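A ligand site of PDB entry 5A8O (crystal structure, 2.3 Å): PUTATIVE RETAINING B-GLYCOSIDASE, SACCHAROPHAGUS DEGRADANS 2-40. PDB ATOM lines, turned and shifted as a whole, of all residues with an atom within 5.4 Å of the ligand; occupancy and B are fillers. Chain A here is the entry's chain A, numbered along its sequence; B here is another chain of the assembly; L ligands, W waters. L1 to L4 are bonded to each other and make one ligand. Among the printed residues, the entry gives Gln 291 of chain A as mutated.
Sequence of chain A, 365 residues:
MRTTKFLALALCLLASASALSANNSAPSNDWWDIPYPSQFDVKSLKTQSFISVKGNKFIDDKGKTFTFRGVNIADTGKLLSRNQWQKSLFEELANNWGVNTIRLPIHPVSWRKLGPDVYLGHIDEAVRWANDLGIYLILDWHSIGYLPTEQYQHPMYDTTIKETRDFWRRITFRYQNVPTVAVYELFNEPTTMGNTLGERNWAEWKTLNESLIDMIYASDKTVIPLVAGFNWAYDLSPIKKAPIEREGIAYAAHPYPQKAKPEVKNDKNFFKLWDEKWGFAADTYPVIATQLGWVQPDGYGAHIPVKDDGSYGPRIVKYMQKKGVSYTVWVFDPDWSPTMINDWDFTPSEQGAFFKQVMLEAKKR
The side-chain amino group (NZ) of Lys 259 lies within hydrogen-bond range of an oxygen (O3) of LIG L1 (2.8 Å). An oxygen (O5) of LG4 L4 is in hydrogen-bond range of a ring nitrogen (NE2) of His 107, 2.8 Å away. An oxygen (O1) of LG3 L3 is in hydrogen-bond range of the side-chain carboxylate of Glu 189, 2.9 Å away. The backbone NH (N) of Ser 337 sits at hydrogen-bond distance from an oxygen (O2) of LG4 L4 (3.3 Å). The backbone carbonyl oxygen (O) of Ser 337 lies within hydrogen-bond range of an oxygen (O1) of LG4 L4, at 3.0 Å. An oxygen (O1) of LG4 L4 lies within hydrogen-bond range of the side-chain hydroxyl of Ser 337 (3.1 Å). NZ of Lys 261 is in hydrogen-bond range of O1 of LIG L1. O1 of LG3 L3 sits at hydrogen-bond distance from OH of Tyr 256, 3.2 Å away. The indole nitrogen (NE1) of Trp 336 is in hydrogen-bond range of an oxygen (O3) of LG4 L4 (3.2 Å). NE2 of Gln 291 sits at hydrogen-bond distance from O2 of LG3 L3, 3.4 Å away.
The side-chain amino group of Lys 261 sits at hydrogen-bond distance from the backbone carbonyl oxygen of Lys 259 (3.5 Å). OE2 of Glu 189 lies within hydrogen-bond range of OH of Tyr 256 (2.8 Å). The backbone carbonyl oxygen (O) of Ser 337 lies within hydrogen-bond range of the indole nitrogen (NE1) of Trp 330 (3.0 Å). OH of Tyr 256 lies within hydrogen-bond range of NE2 of Gln 291, at 2.7 Å. The side-chain amide oxygen of Gln 153 sits at hydrogen-bond distance from the indole nitrogen of Trp 232. The backbone carbonyl oxygen (O) of Pro 305 lies within hydrogen-bond range of the backbone NH (N) of Gln 258, 3.0 Å away. The side-chain amide nitrogen of Gln 153 sits at hydrogen-bond distance from the side-chain hydroxyl of Tyr 36 of chain B. The backbone carbonyl oxygen of Ile 144 is in hydrogen-bond range of the backbone NH of Gln 153 (3.0 Å).
Merely in contact with the ligand: Ile 144 (3.9 Å), Gln 153 (3.5 Å), Met 156 (3.5 Å), Tyr 157 (3.5 Å), Trp 232 (3.4 Å), Pro 305 (3.4 Å), Trp 330 (3.96 Å), Trp 32 of chain B (3.8 Å) and Tyr 36 of chain B (3.8 Å). Hydrophobic or aromatic side chains that line the ligand: His 107, Ile 144, Met 156, Trp 232, Tyr 256, Pro 305, Trp 330, Trp 336 and Trp 32 of chain B. 17 residues have an atom within 4 Å of the ligand: His 107, Ile 144, Gln 153, Met 156, Tyr 157, Glu 189, Trp 232, Tyr 256, Lys 259, Lys 261, Gln 291, Pro 305, Trp 330, Trp 336, Ser 337, Trp 32 of chain B and Tyr 36 of chain B. The nearest printed residue that does not touch the ligand is Ile 304 (4.01 Å).
Water W1 lies within hydrogen-bond range of O2 of LG3 L3, NE2 of His 142 and OH of Tyr 157. Water W6 lies within hydrogen-bond range of O3 of LG3 L3 (2.6 Å), O of Ser 337 (2.7 Å) and NE1 of Trp 330 (3.4 Å). Water W7 lies within hydrogen-bond range of an oxygen (O2) of LG3 L3, the side-chain amide oxygen (OE1) of Gln 291, the side-chain carboxylate (OE1) of Glu 189 and a ring nitrogen (NE2) of His 142. Water W3 lies within hydrogen-bond range of O of Trp 232, O5 of LG2 L2, NZ of Lys 259 and O of Asn 231. Water W5 lies within hydrogen-bond range of the side-chain hydroxyl (OG) of Ser 337 (2.7 Å) and an oxygen (O2) of LG4 L4 (3.4 Å). Water W2 lies within hydrogen-bond range of O of Ile 304 (2.7 Å) and O2 of LG2 L2 (3.4 Å).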
ATOM      1  N   HIS A 107     -23.245  12.593  24.286  1.00  0.00           N
ATOM      2  CA  HIS A 107     -21.921  12.158  23.871  1.00  0.00           C
ATOM      3  C   HIS A 107     -21.926  10.646  23.625  1.00  0.00           C
ATOM      4  O   HIS A 107     -22.370   9.884  24.476  1.00  0.00           O
ATOM      5  CB  HIS A 107     -20.880  12.491  24.937  1.00  0.00           C
ATOM      6  CG  HIS A 107     -20.605  13.944  25.083  1.00  0.00           C
ATOM      7  ND1 HIS A 107     -21.597  14.882  25.312  1.00  0.00           N
ATOM      8  CD2 HIS A 107     -19.443  14.634  25.068  1.00  0.00           C
ATOM      9  CE1 HIS A 107     -21.058  16.075  25.422  1.00  0.00           C
ATOM     10  NE2 HIS A 107     -19.753  15.954  25.277  1.00  0.00           N
ATOM     11  N   HIS A 142     -23.773  14.258  19.854  1.00  0.00           N
ATOM     12  CA  HIS A 142     -22.702  15.195  20.161  1.00  0.00           C
ATOM     13  C   HIS A 142     -21.337  14.594  19.909  1.00  0.00           C
ATOM     14  O   HIS A 142     -20.647  14.199  20.841  1.00  0.00           O
ATOM     15  CB  HIS A 142     -22.792  15.703  21.601  1.00  0.00           C
ATOM     16  CG  HIS A 142     -22.015  16.968  21.848  1.00  0.00           C
ATOM     17  ND1 HIS A 142     -22.527  18.206  21.579  1.00  0.00           N
ATOM     18  CD2 HIS A 142     -20.750  17.163  22.297  1.00  0.00           C
ATOM     19  CE1 HIS A 142     -21.620  19.129  21.849  1.00  0.00           C
ATOM     20  NE2 HIS A 142     -20.537  18.520  22.298  1.00  0.00           N
ATOM     21  N   ILE A 144     -17.610  15.180  17.389  1.00  0.00           N
ATOM     22  CA  ILE A 144     -16.764  16.186  16.775  1.00  0.00           C
ATOM     23  C   ILE A 144     -15.797  15.396  15.911  1.00  0.00           C
ATOM     24  O   ILE A 144     -15.059  14.537  16.398  1.00  0.00           O
ATOM     25  CB  ILE A 144     -15.976  17.004  17.834  1.00  0.00           C
ATOM     26  CG1 ILE A 144     -16.931  17.671  18.819  1.00  0.00           C
ATOM     27  CG2 ILE A 144     -15.097  18.051  17.170  1.00  0.00           C
ATOM     28  CD1 ILE A 144     -16.259  18.641  19.778  1.00  0.00           C
ATOM     29  N   GLN A 153     -12.120  14.085  17.035  1.00  0.00           N
ATOM     30  CA  GLN A 153     -11.251  14.975  17.784  1.00  0.00           C
ATOM     31  C   GLN A 153     -10.765  14.352  19.099  1.00  0.00           C
ATOM     32  O   GLN A 153      -9.660  14.643  19.532  1.00  0.00           O
ATOM     33  CB  GLN A 153     -11.982  16.301  18.058  1.00  0.00           C
ATOM     34  CG  GLN A 153     -11.276  17.237  19.007  1.00  0.00           C
ATOM     35  CD  GLN A 153     -11.834  18.649  18.980  1.00  0.00           C
ATOM     36  OE1 GLN A 153     -12.024  19.241  17.925  1.00  0.00           O
ATOM     37  NE2 GLN A 153     -12.108  19.196  20.164  1.00  0.00           N
ATOM     38  N   MET A 156     -14.117  10.533  23.438  1.00  0.00           N
ATOM     39  CA  MET A 156     -15.449  10.760  23.994  1.00  0.00           C
ATOM     40  C   MET A 156     -16.476  10.980  22.880  1.00  0.00           C
ATOM     41  O   MET A 156     -17.669  10.796  23.106  1.00  0.00           O
ATOM     42  CB  MET A 156     -15.463  11.944  24.993  1.00  0.00           C
ATOM     43  CG  MET A 156     -15.421  13.332  24.368  1.00  0.00           C
ATOM     44  SD  MET A 156     -15.488  14.674  25.572  1.00  0.00           S
ATOM     45  CE  MET A 156     -13.826  14.619  26.252  1.00  0.00           C
ATOM     46  N   TYR A 157     -16.003  11.349  21.693  1.00  0.00           N
ATOM     47  CA  TYR A 157     -16.870  11.632  20.548  1.00  0.00           C
ATOM     48  C   TYR A 157     -16.922  10.460  19.548  1.00  0.00           C
ATOM     49  O   TYR A 157     -17.619  10.534  18.531  1.00  0.00           O
ATOM     50  CB  TYR A 157     -16.386  12.879  19.807  1.00  0.00           C
ATOM     51  CG  TYR A 157     -16.221  14.113  20.663  1.00  0.00           C
ATOM     52  CD1 TYR A 157     -17.299  14.659  21.357  1.00  0.00           C
ATOM     53  CD2 TYR A 157     -14.974  14.720  20.794  1.00  0.00           C
ATOM     54  CE1 TYR A 157     -17.134  15.784  22.155  1.00  0.00           C
ATOM     55  CE2 TYR A 157     -14.800  15.834  21.587  1.00  0.00           C
ATOM     56  CZ  TYR A 157     -15.870  16.371  22.253  1.00  0.00           C
ATOM     57  OH  TYR A 157     -15.662  17.491  23.032  1.00  0.00           O
ATOM     58  N   GLU A 189     -20.530  18.685  15.506  1.00  0.00           N
ATOM     59  CA  GLU A 189     -19.518  19.496  14.829  1.00  0.00           C
ATOM     60  C   GLU A 189     -18.689  18.752  13.780  1.00  0.00           C
ATOM     61  O   GLU A 189     -17.671  18.153  14.110  1.00  0.00           O
ATOM     62  CB  GLU A 189     -18.590  20.157  15.872  1.00  0.00           C
ATOM     63  CG  GLU A 189     -19.287  21.315  16.600  1.00  0.00           C
ATOM     64  CD  GLU A 189     -18.385  22.072  17.575  1.00  0.00           C
ATOM     65  OE1 GLU A 189     -17.400  21.505  18.074  1.00  0.00           O
ATOM     66  OE2 GLU A 189     -18.705  23.249  17.844  1.00  0.00           O
ATOM     67  N   ASN A 231     -15.704  23.018   9.476  1.00  0.00           N
ATOM     68  CA  ASN A 231     -15.059  23.962  10.379  1.00  0.00           C
ATOM     69  C   ASN A 231     -15.769  24.024  11.730  1.00  0.00           C
ATOM     70  O   ASN A 231     -16.089  25.103  12.235  1.00  0.00           O
ATOM     71  CB  ASN A 231     -14.932  25.359   9.743  1.00  0.00           C
ATOM     72  CG  ASN A 231     -13.872  26.200  10.417  1.00  0.00           C
ATOM     73  OD1 ASN A 231     -13.260  25.767  11.393  1.00  0.00           O
ATOM     74  ND2 ASN A 231     -13.625  27.380   9.899  1.00  0.00           N
ATOM     75  N   TRP A 232     -15.998  22.846  12.320  1.00  0.00           N
ATOM     76  CA  TRP A 232     -16.718  22.727  13.575  1.00  0.00           C
ATOM     77  C   TRP A 232     -18.101  23.436  13.510  1.00  0.00           C
ATOM     78  O   TRP A 232     -18.422  24.299  14.319  1.00  0.00           O
ATOM     79  CB  TRP A 232     -15.876  23.253  14.751  1.00  0.00           C
ATOM     80  CG  TRP A 232     -14.660  22.439  15.167  1.00  0.00           C
ATOM     81  CD1 TRP A 232     -14.605  21.522  16.192  1.00  0.00           C
ATOM     82  CD2 TRP A 232     -13.321  22.524  14.630  1.00  0.00           C
ATOM     83  NE1 TRP A 232     -13.325  21.023  16.314  1.00  0.00           N
ATOM     84  CE2 TRP A 232     -12.526  21.606  15.355  1.00  0.00           C
ATOM     85  CE3 TRP A 232     -12.729  23.256  13.604  1.00  0.00           C
ATOM     86  CZ2 TRP A 232     -11.146  21.429  15.083  1.00  0.00           C
ATOM     87  CZ3 TRP A 232     -11.368  23.064  13.329  1.00  0.00           C
ATOM     88  CH2 TRP A 232     -10.596  22.165  14.076  1.00  0.00           C
ATOM     89  N   TYR A 256     -18.564  30.966  17.363  1.00  0.00           N
ATOM     90  CA  TYR A 256     -17.736  31.391  18.497  1.00  0.00           C
ATOM     91  C   TYR A 256     -16.961  32.673  18.139  1.00  0.00           C
ATOM     92  O   TYR A 256     -16.669  32.925  16.959  1.00  0.00           O
ATOM     93  CB  TYR A 256     -16.747  30.294  18.896  1.00  0.00           C
ATOM     94  CG  TYR A 256     -17.372  28.946  19.164  1.00  0.00           C
ATOM     95  CD1 TYR A 256     -18.089  28.700  20.336  1.00  0.00           C
ATOM     96  CD2 TYR A 256     -17.257  27.917  18.248  1.00  0.00           C
ATOM     97  CE1 TYR A 256     -18.662  27.465  20.578  1.00  0.00           C
ATOM     98  CE2 TYR A 256     -17.825  26.683  18.478  1.00  0.00           C
ATOM     99  CZ  TYR A 256     -18.530  26.457  19.649  1.00  0.00           C
ATOM    100  OH  TYR A 256     -19.075  25.211  19.841  1.00  0.00           O
ATOM    101  N   GLN A 258     -13.962  33.800  18.132  1.00  0.00           N
ATOM    102  CA  GLN A 258     -12.697  33.847  17.411  1.00  0.00           C
ATOM    103  C   GLN A 258     -12.718  33.125  16.059  1.00  0.00           C
ATOM    104  O   GLN A 258     -11.676  32.987  15.436  1.00  0.00           O
ATOM    105  CB  GLN A 258     -11.571  33.313  18.295  1.00  0.00           C
ATOM    106  CG  GLN A 258     -11.274  34.188  19.501  1.00  0.00           C
ATOM    107  CD  GLN A 258     -10.250  33.550  20.426  1.00  0.00           C
ATOM    108  OE1 GLN A 258     -10.528  32.544  21.066  1.00  0.00           O
ATOM    109  NE2 GLN A 258      -9.051  34.127  20.490  1.00  0.00           N
ATOM    110  N   LYS A 259     -13.892  32.683  15.615  1.00  0.00           N
ATOM    111  CA  LYS A 259     -14.021  32.019  14.302  1.00  0.00           C
ATOM    112  C   LYS A 259     -13.756  33.014  13.184  1.00  0.00           C
ATOM    113  O   LYS A 259     -12.902  32.773  12.328  1.00  0.00           O
ATOM    114  CB  LYS A 259     -15.412  31.406  14.128  1.00  0.00           C
ATOM    115  CG  LYS A 259     -15.778  30.286  15.094  1.00  0.00           C
ATOM    116  CD  LYS A 259     -14.861  29.069  15.037  1.00  0.00           C
ATOM    117  CE  LYS A 259     -14.905  28.402  13.695  1.00  0.00           C
ATOM    118  NZ  LYS A 259     -14.260  27.069  13.711  1.00  0.00           N
ATOM    119  N   LYS A 261     -12.094  36.367  11.953  1.00  0.00           N
ATOM    120  CA  LYS A 261     -10.878  37.027  12.385  1.00  0.00           C
ATOM    121  C   LYS A 261     -10.621  38.342  11.631  1.00  0.00           C
ATOM    122  O   LYS A 261      -9.626  38.461  10.915  1.00  0.00           O
ATOM    123  CB  LYS A 261      -9.674  36.082  12.224  1.00  0.00           C
ATOM    124  CG  LYS A 261      -9.881  34.663  12.737  1.00  0.00           C
ATOM    125  CD  LYS A 261      -8.635  34.129  13.436  1.00  0.00           C
ATOM    126  CE  LYS A 261      -8.488  32.616  13.347  1.00  0.00           C
ATOM    127  NZ  LYS A 261      -9.753  31.854  13.525  1.00  0.00           N
ATOM    128  N   GLN A 291     -24.441  26.187  19.473  1.00  0.00           N
ATOM    129  CA  GLN A 291     -23.343  26.433  20.384  1.00  0.00           C
ATOM    130  C   GLN A 291     -22.755  27.783  20.089  1.00  0.00           C
ATOM    131  O   GLN A 291     -22.471  28.091  18.943  1.00  0.00           O
ATOM    132  CB  GLN A 291     -22.231  25.372  20.283  1.00  0.00           C
ATOM    133  CG  GLN A 291     -22.370  24.277  21.295  1.00  0.00           C
ATOM    134  CD  GLN A 291     -21.223  23.301  21.332  1.00  0.00           C
ATOM    135  OE1 GLN A 291     -21.365  22.174  20.889  1.00  0.00           O
ATOM    136  NE2 GLN A 291     -20.104  23.715  21.889  1.00  0.00           N
ATOM    137  N   ILE A 304      -8.990  28.929  22.592  1.00  0.00           N
ATOM    138  CA  ILE A 304      -9.469  29.239  21.249  1.00  0.00           C
ATOM    139  C   ILE A 304     -10.570  28.220  20.934  1.00  0.00           C
ATOM    140  O   ILE A 304     -10.411  27.052  21.278  1.00  0.00           O
ATOM    141  CB  ILE A 304      -8.305  29.158  20.208  1.00  0.00           C
ATOM    142  CG1 ILE A 304      -7.416  30.402  20.318  1.00  0.00           C
ATOM    143  CG2 ILE A 304      -8.825  29.046  18.784  1.00  0.00           C
ATOM    144  CD1 ILE A 304      -6.079  30.279  19.608  1.00  0.00           C
ATOM    145  N   PRO A 305     -11.688  28.644  20.305  1.00  0.00           N
ATOM    146  CA  PRO A 305     -12.031  29.967  19.797  1.00  0.00           C
ATOM    147  C   PRO A 305     -13.029  30.734  20.674  1.00  0.00           C
ATOM    148  O   PRO A 305     -13.809  31.528  20.144  1.00  0.00           O
ATOM    149  CB  PRO A 305     -12.708  29.622  18.484  1.00  0.00           C
ATOM    150  CG  PRO A 305     -13.497  28.374  18.831  1.00  0.00           C
ATOM    151  CD  PRO A 305     -12.720  27.668  19.919  1.00  0.00           C
ATOM    152  N   TRP A 330     -23.747  27.810  25.172  1.00  0.00           N
ATOM    153  CA  TRP A 330     -22.909  26.767  25.755  1.00  0.00           C
ATOM    154  C   TRP A 330     -22.071  27.423  26.854  1.00  0.00           C
ATOM    155  O   TRP A 330     -21.362  28.388  26.549  1.00  0.00           O
ATOM    156  CB  TRP A 330     -21.980  26.185  24.662  1.00  0.00           C
ATOM    157  CG  TRP A 330     -21.028  25.127  25.165  1.00  0.00           C
ATOM    158  CD1 TRP A 330     -19.821  25.327  25.776  1.00  0.00           C
ATOM    159  CD2 TRP A 330     -21.210  23.705  25.125  1.00  0.00           C
ATOM    160  NE1 TRP A 330     -19.248  24.127  26.120  1.00  0.00           N
ATOM    161  CE2 TRP A 330     -20.088  23.112  25.723  1.00  0.00           C
ATOM    162  CE3 TRP A 330     -22.234  22.866  24.645  1.00  0.00           C
ATOM    163  CZ2 TRP A 330     -19.953  21.728  25.849  1.00  0.00           C
ATOM    164  CZ3 TRP A 330     -22.093  21.489  24.767  1.00  0.00           C
ATOM    165  CH2 TRP A 330     -20.956  20.939  25.361  1.00  0.00           C
ATOM    166  N   ASP A 335     -18.677  23.044  35.486  1.00  0.00           N
ATOM    167  CA  ASP A 335     -17.403  22.352  35.242  1.00  0.00           C
ATOM    168  C   ASP A 335     -16.963  22.498  33.792  1.00  0.00           C
ATOM    169  O   ASP A 335     -15.803  22.788  33.528  1.00  0.00           O
ATOM    170  CB  ASP A 335     -17.543  20.865  35.576  1.00  0.00           C
ATOM    171  CG  ASP A 335     -18.110  20.640  36.961  1.00  0.00           C
ATOM    172  OD1 ASP A 335     -17.568  21.221  37.910  1.00  0.00           O
ATOM    173  OD2 ASP A 335     -19.099  19.889  37.090  1.00  0.00           O
ATOM    174  N   TRP A 336     -17.891  22.299  32.861  1.00  0.00           N
ATOM    175  CA  TRP A 336     -17.607  22.443  31.427  1.00  0.00           C
ATOM    176  C   TRP A 336     -17.530  23.903  31.035  1.00  0.00           C
ATOM    177  O   TRP A 336     -18.267  24.731  31.573  1.00  0.00           O
ATOM    178  CB  TRP A 336     -18.697  21.740  30.608  1.00  0.00           C
ATOM    179  CG  TRP A 336     -18.612  20.243  30.649  1.00  0.00           C
ATOM    180  CD1 TRP A 336     -17.809  19.476  31.465  1.00  0.00           C
ATOM    181  CD2 TRP A 336     -19.365  19.326  29.853  1.00  0.00           C
ATOM    182  NE1 TRP A 336     -18.007  18.132  31.202  1.00  0.00           N
ATOM    183  CE2 TRP A 336     -18.959  18.023  30.220  1.00  0.00           C
ATOM    184  CE3 TRP A 336     -20.339  19.482  28.871  1.00  0.00           C
ATOM    185  CZ2 TRP A 336     -19.495  16.892  29.632  1.00  0.00           C
ATOM    186  CZ3 TRP A 336     -20.875  18.357  28.292  1.00  0.00           C
ATOM    187  CH2 TRP A 336     -20.451  17.074  28.670  1.00  0.00           C
ATOM    188  N   SER A 337     -16.629  24.227  30.100  1.00  0.00           N
ATOM    189  CA  SER A 337     -16.366  25.617  29.756  1.00  0.00           C
ATOM    190  C   SER A 337     -16.677  25.921  28.282  1.00  0.00           C
ATOM    191  O   SER A 337     -16.669  24.996  27.458  1.00  0.00           O
ATOM    192  CB  SER A 337     -14.913  25.939  30.058  1.00  0.00           C
ATOM    193  OG  SER A 337     -14.075  25.121  29.253  1.00  0.00           O
ATOM    194  N   PRO A 338     -16.948  27.205  27.949  1.00  0.00           N
ATOM    195  CA  PRO A 338     -17.137  28.333  28.854  1.00  0.00           C
ATOM    196  C   PRO A 338     -18.439  28.180  29.633  1.00  0.00           C
ATOM    197  O   PRO A 338     -19.459  27.806  29.044  1.00  0.00           O
ATOM    198  CB  PRO A 338     -17.223  29.543  27.906  1.00  0.00           C
ATOM    199  CG  PRO A 338     -17.724  28.964  26.620  1.00  0.00           C
ATOM    200  CD  PRO A 338     -17.080  27.614  26.538  1.00  0.00           C
ATOM    201  N   TRP B  31     -15.085  10.253  31.696  1.00  0.00           N
ATOM    202  CA  TRP B  31     -14.646  10.293  30.306  1.00  0.00           C
ATOM    203  C   TRP B  31     -14.358  11.702  29.793  1.00  0.00           C
ATOM    204  O   TRP B  31     -13.524  11.880  28.905  1.00  0.00           O
ATOM    205  CB  TRP B  31     -15.659   9.611  29.370  1.00  0.00           C
ATOM    206  CG  TRP B  31     -17.067   9.989  29.600  1.00  0.00           C
ATOM    207  CD1 TRP B  31     -17.986   9.280  30.311  1.00  0.00           C
ATOM    208  CD2 TRP B  31     -17.747  11.139  29.102  1.00  0.00           C
ATOM    209  NE1 TRP B  31     -19.185   9.931  30.309  1.00  0.00           N
ATOM    210  CE2 TRP B  31     -19.071  11.075  29.577  1.00  0.00           C
ATOM    211  CE3 TRP B  31     -17.367  12.223  28.307  1.00  0.00           C
ATOM    212  CZ2 TRP B  31     -20.030  12.064  29.277  1.00  0.00           C
ATOM    213  CZ3 TRP B  31     -18.319  13.207  28.011  1.00  0.00           C
ATOM    214  CH2 TRP B  31     -19.630  13.110  28.498  1.00  0.00           C
ATOM    215  N   TRP B  32     -15.022  12.706  30.363  1.00  0.00           N
ATOM    216  CA  TRP B  32     -14.783  14.093  29.958  1.00  0.00           C
ATOM    217  C   TRP B  32     -13.444  14.644  30.473  1.00  0.00           C
ATOM    218  O   TRP B  32     -13.023  15.710  30.056  1.00  0.00           O
ATOM    219  CB  TRP B  32     -15.942  15.012  30.371  1.00  0.00           C
ATOM    220  CG  TRP B  32     -16.200  15.065  31.831  1.00  0.00           C
ATOM    221  CD1 TRP B  32     -15.655  15.922  32.738  1.00  0.00           C
ATOM    222  CD2 TRP B  32     -17.081  14.221  32.562  1.00  0.00           C
ATOM    223  NE1 TRP B  32     -16.144  15.665  33.993  1.00  0.00           N
ATOM    224  CE2 TRP B  32     -17.013  14.610  33.912  1.00  0.00           C
ATOM    225  CE3 TRP B  32     -17.910  13.148  32.205  1.00  0.00           C
ATOM    226  CZ2 TRP B  32     -17.745  13.979  34.908  1.00  0.00           C
ATOM    227  CZ3 TRP B  32     -18.648  12.510  33.206  1.00  0.00           C
ATOM    228  CH2 TRP B  32     -18.550  12.935  34.534  1.00  0.00           C
ATOM    229  N   TYR B  36      -6.279  14.947  26.160  1.00  0.00           N
ATOM    230  CA  TYR B  36      -5.876  14.982  24.759  1.00  0.00           C
ATOM    231  C   TYR B  36      -4.421  14.481  24.628  1.00  0.00           C
ATOM    232  O   TYR B  36      -3.629  14.635  25.556  1.00  0.00           O
ATOM    233  CB  TYR B  36      -6.028  16.395  24.189  1.00  0.00           C
ATOM    234  CG  TYR B  36      -7.443  16.725  23.798  1.00  0.00           C
ATOM    235  CD1 TYR B  36      -8.369  17.199  24.722  1.00  0.00           C
ATOM    236  CD2 TYR B  36      -7.873  16.538  22.492  1.00  0.00           C
ATOM    237  CE1 TYR B  36      -9.682  17.487  24.354  1.00  0.00           C
ATOM    238  CE2 TYR B  36      -9.171  16.823  22.116  1.00  0.00           C
ATOM    239  CZ  TYR B  36     -10.075  17.289  23.034  1.00  0.00           C
ATOM    240  OH  TYR B  36     -11.364  17.552  22.636  1.00  0.00           O
HETATM  241  C1  LIG L   1     -10.657  27.855  14.072  1.00  0.00           C
HETATM  242  C2  LIG L   1     -10.906  27.267  15.446  1.00  0.00           C
HETATM  243  C3  LIG L   1     -10.086  25.995  15.590  1.00  0.00           C
HETATM  244  C4  LIG L   1      -8.637  26.137  15.155  1.00  0.00           C
HETATM  245  C5  LIG L   1      -8.051  24.751  14.936  1.00  0.00           C
HETATM  246  C6  LIG L   1      -9.165  28.143  14.025  1.00  0.00           C
HETATM  247  O1  LIG L   1      -8.855  28.947  12.895  1.00  0.00           O
HETATM  248  O2  LIG L   1     -11.429  29.037  13.872  1.00  0.00           O
HETATM  249  O3  LIG L   1     -12.298  27.016  15.645  1.00  0.00           O
HETATM  250  O4  LIG L   1     -10.066  25.645  16.966  1.00  0.00           O
HETATM  251  O5  LIG L   1      -8.494  26.892  13.950  1.00  0.00           O
HETATM  252  O6  LIG L   1      -6.643  24.809  15.197  1.00  0.00           O
HETATM  253  C1  LG2 L   2     -10.547  24.036  18.643  1.00  0.00           C
HETATM  254  C2  LG2 L   2     -11.572  23.043  19.151  1.00  0.00           C
HETATM  255  C3  LG2 L   2     -12.935  23.712  19.235  1.00  0.00           C
HETATM  256  C4  LG2 L   2     -13.272  24.332  17.885  1.00  0.00           C
HETATM  257  C5  LG2 L   2     -14.607  25.072  17.887  1.00  0.00           C
HETATM  258  C6  LG2 L   2     -11.004  24.652  17.335  1.00  0.00           C
HETATM  259  O1  LG2 L   2      -9.292  23.380  18.458  1.00  0.00           O
HETATM  260  O2  LG2 L   2     -11.151  22.632  20.438  1.00  0.00           O
HETATM  261  O3  LG2 L   2     -13.929  22.746  19.570  1.00  0.00           O
HETATM  262  O4  LG2 L   2     -12.260  25.267  17.500  1.00  0.00           O
HETATM  263  O5  LG2 L   2     -14.704  25.798  16.661  1.00  0.00           O
HETATM  264  C1  LG3 L   3     -15.797  22.346  21.048  1.00  0.00           C
HETATM  265  C2  LG3 L   3     -16.249  22.355  22.500  1.00  0.00           C
HETATM  266  C3  LG3 L   3     -15.220  21.729  23.430  1.00  0.00           C
HETATM  267  C4  LG3 L   3     -13.802  22.220  23.118  1.00  0.00           C
HETATM  268  C5  LG3 L   3     -12.733  21.549  23.984  1.00  0.00           C
HETATM  269  C6  LG3 L   3     -14.353  22.820  20.932  1.00  0.00           C
HETATM  270  O1  LG3 L   3     -16.678  23.163  20.277  1.00  0.00           O
HETATM  271  O2  LG3 L   3     -17.478  21.629  22.644  1.00  0.00           O
HETATM  272  O3  LG3 L   3     -15.616  22.101  24.748  1.00  0.00           O
HETATM  273  O4  LG3 L   3     -13.512  21.996  21.729  1.00  0.00           O
HETATM  274  O5  LG3 L   3     -11.558  21.307  23.210  1.00  0.00           O
HETATM  275  C1  LG4 L   4     -15.443  21.787  27.091  1.00  0.00           C
HETATM  276  C2  LG4 L   4     -15.106  20.740  28.150  1.00  0.00           C
HETATM  277  C3  LG4 L   4     -16.074  19.570  28.008  1.00  0.00           C
HETATM  278  C4  LG4 L   4     -15.990  19.020  26.583  1.00  0.00           C
HETATM  279  C5  LG4 L   4     -16.879  17.819  26.334  1.00  0.00           C
HETATM  280  C6  LG4 L   4     -15.386  21.114  25.736  1.00  0.00           C
HETATM  281  O1  LG4 L   4     -14.528  22.892  27.104  1.00  0.00           O
HETATM  282  O2  LG4 L   4     -15.176  21.342  29.444  1.00  0.00           O
HETATM  283  O3  LG4 L   4     -15.745  18.536  28.937  1.00  0.00           O
HETATM  284  O4  LG4 L   4     -16.325  20.053  25.667  1.00  0.00           O
HETATM  285  O5  LG4 L   4     -18.128  18.202  25.809  1.00  0.00           O
HETATM  286  O   HOH W   1     -17.985  19.244  23.296  1.00  0.00           O
HETATM  287  O   HOH W   2     -12.059  25.242  22.444  1.00  0.00           O
HETATM  288  O   HOH W   3     -17.053  26.478  15.304  1.00  0.00           O
HETATM  289  O   HOH W   4     -15.891  25.662  21.285  1.00  0.00           O
HETATM  290  O   HOH W   5     -12.366  23.178  29.923  1.00  0.00           O
HETATM  291  O   HOH W   6     -16.163  24.596  24.822  1.00  0.00           O
HETATM  292  O   HOH W   7     -18.898  20.974  20.428  1.00  0.00           O
HETATM  293  O   HOH W   8      -6.916  25.270  19.065  1.00  0.00           O
HETATM  294  O   HOH W   9     -10.591  29.209  10.229  1.00  0.00           O
